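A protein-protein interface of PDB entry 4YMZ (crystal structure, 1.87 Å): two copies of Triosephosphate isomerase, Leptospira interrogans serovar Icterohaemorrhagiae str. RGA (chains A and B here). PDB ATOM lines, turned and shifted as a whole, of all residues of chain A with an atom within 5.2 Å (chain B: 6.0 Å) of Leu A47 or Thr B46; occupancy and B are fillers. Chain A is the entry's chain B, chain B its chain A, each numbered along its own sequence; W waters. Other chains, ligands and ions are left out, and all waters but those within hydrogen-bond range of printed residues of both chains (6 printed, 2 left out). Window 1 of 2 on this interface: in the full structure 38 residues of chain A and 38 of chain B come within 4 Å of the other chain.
The backbone NH of Ser B81 sits at hydrogen-bond distance from the side-chain amide oxygen of Gln B84 (3.0 Å). The backbone carbonyl oxygen of Pro B44 is in hydrogen-bond range of the side-chain amide nitrogen of Gln B66.
The side-chain amide oxygen (OE1) of Gln B66 lies within hydrogen-bond range of the backbone NH (N) of Gly A78 (2.6 Å). The side-chain hydroxyl of Ser A45 lies within hydrogen-bond range of the side-chain amide nitrogen of Gln B84 (3.0 Å).
Water W6 lies within hydrogen-bond range of the side-chain hydroxyl of Thr B80 (2.6 Å), the backbone NH of Leu A47 (2.9 Å) and the backbone NH of Thr A46 (3.2 Å). Water W5 bridges the backbone NH of Thr B46 and the backbone carbonyl oxygen of Gly A78. Water W2 lies within hydrogen-bond range of the backbone carbonyl oxygen (O) of Gln B84 (2.8 Å) and a ring nitrogen (NE2) of His A48 (2.9 Å). Water W4 lies within hydrogen-bond range of OG1 of Thr A80, N of Leu B47 and N of Thr B46. Water W3 lies within hydrogen-bond range of the side-chain carboxylate (OE1) of Glu B50 (2.8 Å) and the backbone carbonyl oxygen (O) of Leu A47 (3.0 Å). Water W1 lies within hydrogen-bond range of ND2 of Asn B67 and O of Gly A78.
Hydrophobic or aromatic side chains of chain A that line the printed part of chain B: Leu A47, His A48 and Leu A49. Printed residues of chain B that touch a printed residue of chain A: Thr B46, Leu B47, Leu B49, Gln B66, Gln B84 and Ile B88. Among the printed residues, no Asp or Glu carboxylate lies within 4 Å of a Lys or Arg side-chain nitrogen of the other chain.
Leu A47 touches just these residues of chain B: Thr B46, Leu B49, Gln B84 and Ile B88. Of the printed residues of chain A, Gln B84 touches Ser A45, Leu A47 and His A48. Of the printed residues of chain B, Ser A45 touches Gln B84 (3.0 Å). Printed residues of chain B within 4 Å of Gly A78: Gln B66 (2.6 Å). Of the printed residues of chain A, Gln B66 touches Gly A78. Ala B65 touches none of the printed residues of chain A. Asn B67 touches none of the printed residues of chain A. The nearest residue of chain B that does not touch Leu A47 is Glu B50 (4.1 Å).
Among the printed residues, pairs that only touch across the chains: Leu A47 with Gln B84 (3.5 Å), His A48 with Gln B84 (3.7 Å), Leu A47 with Thr B46 (3.7 Å), Thr A46 with Leu B47 (3.7 Å), Leu A47 with Leu B49 (3.7 Å), Leu A49 with Leu B47 (3.8 Å) and Leu A47 with Ile B88 (3.9 Å).
Thr A46 touches Leu B47, and with the chains exchanged Leu A47 touches Thr B46. Leu A47 touches Leu B49, and with the chains exchanged Leu A49 touches Leu B47. 6 positions are printed for both chains. Of the 9 pairs that touch across the chains among the printed residues, 4 have their exchanged pair printed and touching as well.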
ATOM      1  N   SER A  45      15.045  -8.331  -6.167  1.00  0.00           N
ATOM      2  CA  SER A  45      14.682  -6.865  -6.005  1.00  0.00           C
ATOM      3  C   SER A  45      15.919  -6.006  -6.169  1.00  0.00           C
ATOM      4  O   SER A  45      17.041  -6.401  -5.827  1.00  0.00           O
ATOM      5  CB  SER A  45      14.110  -6.555  -4.622  1.00  0.00           C
ATOM      6  OG  SER A  45      12.864  -7.184  -4.414  1.00  0.00           O
ATOM      7  N   THR A  46      15.738  -4.804  -6.683  1.00  0.00           N
ATOM      8  CA  THR A  46      16.943  -3.987  -6.981  1.00  0.00           C
ATOM      9  C   THR A  46      17.773  -3.703  -5.743  1.00  0.00           C
ATOM     10  O   THR A  46      18.968  -3.608  -5.822  1.00  0.00           O
ATOM     11  CB  THR A  46      16.502  -2.678  -7.641  1.00  0.00           C
ATOM     12  OG1 THR A  46      15.936  -3.015  -8.928  1.00  0.00           O
ATOM     13  CG2 THR A  46      17.687  -1.731  -7.949  1.00  0.00           C
ATOM     14  N   LEU A  47      17.112  -3.500  -4.624  1.00  0.00           N
ATOM     15  CA  LEU A  47      17.810  -3.282  -3.336  1.00  0.00           C
ATOM     16  C   LEU A  47      18.832  -4.427  -2.938  1.00  0.00           C
ATOM     17  O   LEU A  47      19.762  -4.192  -2.149  1.00  0.00           O
ATOM     18  CB  LEU A  47      16.750  -3.198  -2.261  1.00  0.00           C
ATOM     19  CG  LEU A  47      17.247  -2.685  -0.922  1.00  0.00           C
ATOM     20  CD1 LEU A  47      17.470  -1.204  -0.955  1.00  0.00           C
ATOM     21  CD2 LEU A  47      16.281  -2.940   0.211  1.00  0.00           C
ATOM     22  N   HIS A  48      18.611  -5.629  -3.454  1.00  0.00           N
ATOM     23  CA  HIS A  48      19.403  -6.854  -3.151  1.00  0.00           C
ATOM     24  C   HIS A  48      20.281  -7.280  -4.274  1.00  0.00           C
ATOM     25  O   HIS A  48      20.998  -8.292  -4.178  1.00  0.00           O
ATOM     26  CB  HIS A  48      18.429  -7.968  -2.925  1.00  0.00           C
ATOM     27  CG  HIS A  48      17.444  -7.665  -1.846  1.00  0.00           C
ATOM     28  ND1 HIS A  48      16.228  -8.320  -1.753  1.00  0.00           N
ATOM     29  CD2 HIS A  48      17.448  -6.738  -0.869  1.00  0.00           C
ATOM     30  CE1 HIS A  48      15.565  -7.863  -0.708  1.00  0.00           C
ATOM     31  NE2 HIS A  48      16.283  -6.910  -0.154  1.00  0.00           N
ATOM     32  N   LEU A  49      20.284  -6.533  -5.349  1.00  0.00           N
ATOM     33  CA  LEU A  49      20.997  -7.030  -6.535  1.00  0.00           C
ATOM     34  C   LEU A  49      22.477  -7.095  -6.401  1.00  0.00           C
ATOM     35  O   LEU A  49      23.069  -7.979  -6.941  1.00  0.00           O
ATOM     36  CB  LEU A  49      20.710  -6.172  -7.769  1.00  0.00           C
ATOM     37  CG  LEU A  49      19.512  -6.512  -8.647  1.00  0.00           C
ATOM     38  CD1 LEU A  49      19.348  -5.344  -9.661  1.00  0.00           C
ATOM     39  CD2 LEU A  49      19.730  -7.823  -9.364  1.00  0.00           C
ATOM     40  N   GLY A  78      14.907   8.152  -8.055  1.00  0.00           N
ATOM     41  CA  GLY A  78      14.158   6.867  -7.868  1.00  0.00           C
ATOM     42  C   GLY A  78      14.425   5.803  -8.908  1.00  0.00           C
ATOM     43  O   GLY A  78      14.069   4.622  -8.793  1.00  0.00           O
ATOM     44  N   THR A  80      16.865   3.416 -11.642  1.00  0.00           N
ATOM     45  CA  THR A  80      18.118   2.631 -11.795  1.00  0.00           C
ATOM     46  C   THR A  80      18.596   2.703 -13.293  1.00  0.00           C
ATOM     47  O   THR A  80      17.824   2.512 -14.218  1.00  0.00           O
ATOM     48  CB  THR A  80      17.878   1.167 -11.469  1.00  0.00           C
ATOM     49  OG1 THR A  80      17.356   1.056 -10.128  1.00  0.00           O
ATOM     50  CG2 THR A  80      19.215   0.363 -11.556  1.00  0.00           C
ATOM     51  N   PRO B  44      21.001   7.827  -1.513  1.00  0.00           N
ATOM     52  CA  PRO B  44      21.649   7.099  -2.588  1.00  0.00           C
ATOM     53  C   PRO B  44      20.663   6.433  -3.517  1.00  0.00           C
ATOM     54  O   PRO B  44      19.525   6.239  -3.154  1.00  0.00           O
ATOM     55  CB  PRO B  44      22.420   5.963  -1.854  1.00  0.00           C
ATOM     56  CG  PRO B  44      22.442   6.395  -0.423  1.00  0.00           C
ATOM     57  CD  PRO B  44      21.136   7.104  -0.227  1.00  0.00           C
ATOM     58  N   SER B  45      21.148   5.941  -4.664  1.00  0.00           N
ATOM     59  CA  SER B  45      20.286   5.197  -5.594  1.00  0.00           C
ATOM     60  C   SER B  45      19.922   3.917  -4.925  1.00  0.00           C
ATOM     61  O   SER B  45      20.728   3.367  -4.121  1.00  0.00           O
ATOM     62  CB  SER B  45      21.020   4.876  -6.872  1.00  0.00           C
ATOM     63  OG  SER B  45      21.213   6.031  -7.639  1.00  0.00           O
ATOM     64  N   THR B  46      18.762   3.367  -5.241  1.00  0.00           N
ATOM     65  CA  THR B  46      18.354   2.090  -4.610  1.00  0.00           C
ATOM     66  C   THR B  46      19.363   0.946  -4.672  1.00  0.00           C
ATOM     67  O   THR B  46      19.542   0.199  -3.689  1.00  0.00           O
ATOM     68  CB  THR B  46      16.955   1.687  -5.143  1.00  0.00           C
ATOM     69  OG1 THR B  46      16.054   2.666  -4.629  1.00  0.00           O
ATOM     70  CG2 THR B  46      16.473   0.431  -4.494  1.00  0.00           C
ATOM     71  N   LEU B  47      19.976   0.756  -5.838  1.00  0.00           N
ATOM     72  CA  LEU B  47      20.959  -0.308  -6.080  1.00  0.00           C
ATOM     73  C   LEU B  47      22.118  -0.198  -5.085  1.00  0.00           C
ATOM     74  O   LEU B  47      22.740  -1.168  -4.794  1.00  0.00           O
ATOM     75  CB  LEU B  47      21.542  -0.133  -7.512  1.00  0.00           C
ATOM     76  CG  LEU B  47      22.379  -1.258  -8.056  1.00  0.00           C
ATOM     77  CD1 LEU B  47      21.446  -2.420  -8.330  1.00  0.00           C
ATOM     78  CD2 LEU B  47      23.180  -0.942  -9.305  1.00  0.00           C
ATOM     79  N   HIS B  48      22.328   0.988  -4.498  1.00  0.00           N
ATOM     80  CA  HIS B  48      23.481   1.274  -3.658  1.00  0.00           C
ATOM     81  C   HIS B  48      23.144   1.429  -2.172  1.00  0.00           C
ATOM     82  O   HIS B  48      24.058   1.640  -1.359  1.00  0.00           O
ATOM     83  CB  HIS B  48      24.081   2.608  -4.082  1.00  0.00           C
ATOM     84  CG  HIS B  48      24.533   2.629  -5.472  1.00  0.00           C
ATOM     85  ND1 HIS B  48      24.728   3.804  -6.163  1.00  0.00           N
ATOM     86  CD2 HIS B  48      24.770   1.617  -6.345  1.00  0.00           C
ATOM     87  CE1 HIS B  48      25.158   3.513  -7.377  1.00  0.00           C
ATOM     88  NE2 HIS B  48      25.163   2.207  -7.518  1.00  0.00           N
ATOM     89  N   LEU B  49      21.880   1.361  -1.824  1.00  0.00           N
ATOM     90  CA  LEU B  49      21.429   1.669  -0.476  1.00  0.00           C
ATOM     91  C   LEU B  49      21.981   0.695   0.556  1.00  0.00           C
ATOM     92  O   LEU B  49      22.326   1.145   1.633  1.00  0.00           O
ATOM     93  CB  LEU B  49      19.885   1.601  -0.386  1.00  0.00           C
ATOM     94  CG  LEU B  49      19.200   2.890  -0.775  1.00  0.00           C
ATOM     95  CD1 LEU B  49      17.688   2.633  -0.846  1.00  0.00           C
ATOM     96  CD2 LEU B  49      19.553   3.935   0.319  1.00  0.00           C
ATOM     97  N   GLU B  50      21.983  -0.615   0.293  1.00  0.00           N
ATOM     98  CA  GLU B  50      22.481  -1.566   1.280  1.00  0.00           C
ATOM     99  C   GLU B  50      23.961  -1.247   1.620  1.00  0.00           C
ATOM    100  O   GLU B  50      24.331  -1.123   2.755  1.00  0.00           O
ATOM    101  CB  GLU B  50      22.391  -3.022   0.804  1.00  0.00           C
ATOM    102  CG  GLU B  50      22.774  -3.985   1.955  1.00  0.00           C
ATOM    103  CD  GLU B  50      23.120  -5.390   1.527  1.00  0.00           C
ATOM    104  OE1 GLU B  50      22.998  -5.757   0.300  1.00  0.00           O
ATOM    105  OE2 GLU B  50      23.487  -6.140   2.441  1.00  0.00           O
ATOM    106  N   ALA B  65      15.681   6.658   1.183  1.00  0.00           N
ATOM    107  CA  ALA B  65      15.450   6.076  -0.180  1.00  0.00           C
ATOM    108  C   ALA B  65      14.758   7.092  -1.046  1.00  0.00           C
ATOM    109  O   ALA B  65      13.978   7.922  -0.543  1.00  0.00           O
ATOM    110  CB  ALA B  65      14.576   4.849  -0.131  1.00  0.00           C
ATOM    111  N   GLN B  66      15.014   6.988  -2.347  1.00  0.00           N
ATOM    112  CA  GLN B  66      14.491   7.951  -3.335  1.00  0.00           C
ATOM    113  C   GLN B  66      13.038   7.727  -3.782  1.00  0.00           C
ATOM    114  O   GLN B  66      12.399   8.627  -4.287  1.00  0.00           O
ATOM    115  CB  GLN B  66      15.415   7.946  -4.543  1.00  0.00           C
ATOM    116  CG  GLN B  66      16.734   8.690  -4.330  1.00  0.00           C
ATOM    117  CD  GLN B  66      17.626   8.529  -5.553  1.00  0.00           C
ATOM    118  OE1 GLN B  66      17.138   8.455  -6.703  1.00  0.00           O
ATOM    119  NE2 GLN B  66      18.916   8.580  -5.346  1.00  0.00           N
ATOM    120  N   ASN B  67      12.531   6.534  -3.495  1.00  0.00           N
ATOM    121  CA  ASN B  67      11.186   6.165  -3.848  1.00  0.00           C
ATOM    122  C   ASN B  67      10.880   4.804  -3.239  1.00  0.00           C
ATOM    123  O   ASN B  67      11.791   4.083  -2.852  1.00  0.00           O
ATOM    124  CB  ASN B  67      11.166   6.005  -5.335  1.00  0.00           C
ATOM    125  CG  ASN B  67       9.785   5.707  -5.846  1.00  0.00           C
ATOM    126  OD1 ASN B  67       8.820   6.338  -5.430  1.00  0.00           O
ATOM    127  ND2 ASN B  67       9.692   4.722  -6.683  1.00  0.00           N
ATOM    128  N   THR B  80      10.233  -1.232  -4.800  1.00  0.00           N
ATOM    129  CA  THR B  80      10.924  -1.410  -3.469  1.00  0.00           C
ATOM    130  C   THR B  80       9.922  -1.257  -2.333  1.00  0.00           C
ATOM    131  O   THR B  80       9.197  -0.315  -2.325  1.00  0.00           O
ATOM    132  CB  THR B  80      12.021  -0.321  -3.285  1.00  0.00           C
ATOM    133  OG1 THR B  80      13.024  -0.575  -4.287  1.00  0.00           O
ATOM    134  CG2 THR B  80      12.737  -0.489  -1.965  1.00  0.00           C
ATOM    135  N   SER B  81       9.881  -2.195  -1.412  1.00  0.00           N
ATOM    136  CA  SER B  81       8.987  -2.147  -0.303  1.00  0.00           C
ATOM    137  C   SER B  81       9.594  -1.457   0.888  1.00  0.00           C
ATOM    138  O   SER B  81      10.749  -1.689   1.206  1.00  0.00           O
ATOM    139  CB  SER B  81       8.641  -3.525   0.120  1.00  0.00           C
ATOM    140  OG  SER B  81       7.727  -3.442   1.222  1.00  0.00           O
ATOM    141  N   GLN B  84      11.491  -3.780   3.023  1.00  0.00           N
ATOM    142  CA  GLN B  84      12.841  -4.030   2.638  1.00  0.00           C
ATOM    143  C   GLN B  84      13.784  -2.913   3.044  1.00  0.00           C
ATOM    144  O   GLN B  84      14.925  -3.155   3.387  1.00  0.00           O
ATOM    145  CB  GLN B  84      12.964  -4.260   1.094  1.00  0.00           C
ATOM    146  CG  GLN B  84      12.118  -5.404   0.550  1.00  0.00           C
ATOM    147  CD  GLN B  84      12.077  -5.458  -0.976  1.00  0.00           C
ATOM    148  OE1 GLN B  84      11.954  -4.411  -1.635  1.00  0.00           O
ATOM    149  NE2 GLN B  84      12.212  -6.673  -1.554  1.00  0.00           N
ATOM    150  N   LEU B  85      13.305  -1.712   3.023  1.00  0.00           N
ATOM    151  CA  LEU B  85      14.078  -0.589   3.553  1.00  0.00           C
ATOM    152  C   LEU B  85      14.326  -0.625   5.127  1.00  0.00           C
ATOM    153  O   LEU B  85      15.448  -0.418   5.551  1.00  0.00           O
ATOM    154  CB  LEU B  85      13.378   0.698   3.217  1.00  0.00           C
ATOM    155  CG  LEU B  85      13.370   0.949   1.696  1.00  0.00           C
ATOM    156  CD1 LEU B  85      12.491   2.143   1.406  1.00  0.00           C
ATOM    157  CD2 LEU B  85      14.758   1.138   1.169  1.00  0.00           C
ATOM    158  N   ILE B  88      17.303  -2.828   6.270  1.00  0.00           N
ATOM    159  CA  ILE B  88      18.657  -2.333   6.207  1.00  0.00           C
ATOM    160  C   ILE B  88      18.819  -1.004   6.892  1.00  0.00           C
ATOM    161  O   ILE B  88      19.811  -0.255   6.657  1.00  0.00           O
ATOM    162  CB  ILE B  88      19.127  -2.259   4.730  1.00  0.00           C
ATOM    163  CG1 ILE B  88      18.195  -1.310   3.947  1.00  0.00           C
ATOM    164  CG2 ILE B  88      19.170  -3.689   4.135  1.00  0.00           C
ATOM    165  CD1 ILE B  88      18.778  -0.801   2.666  1.00  0.00           C
HETATM  166  O   HOH W   1      11.898   3.150  -7.540  1.00  0.00           O
HETATM  167  O   HOH W   2      15.642  -5.634   2.416  1.00  0.00           O
HETATM  168  O   HOH W   3      22.449  -5.420  -2.458  1.00  0.00           O
HETATM  169  O   HOH W   4      19.144   2.169  -8.278  1.00  0.00           O
HETATM  170  O   HOH W   5      16.858   4.611  -6.796  1.00  0.00           O
HETATM  171  O   HOH W   6      14.272  -2.888  -4.606  1.00  0.00           O
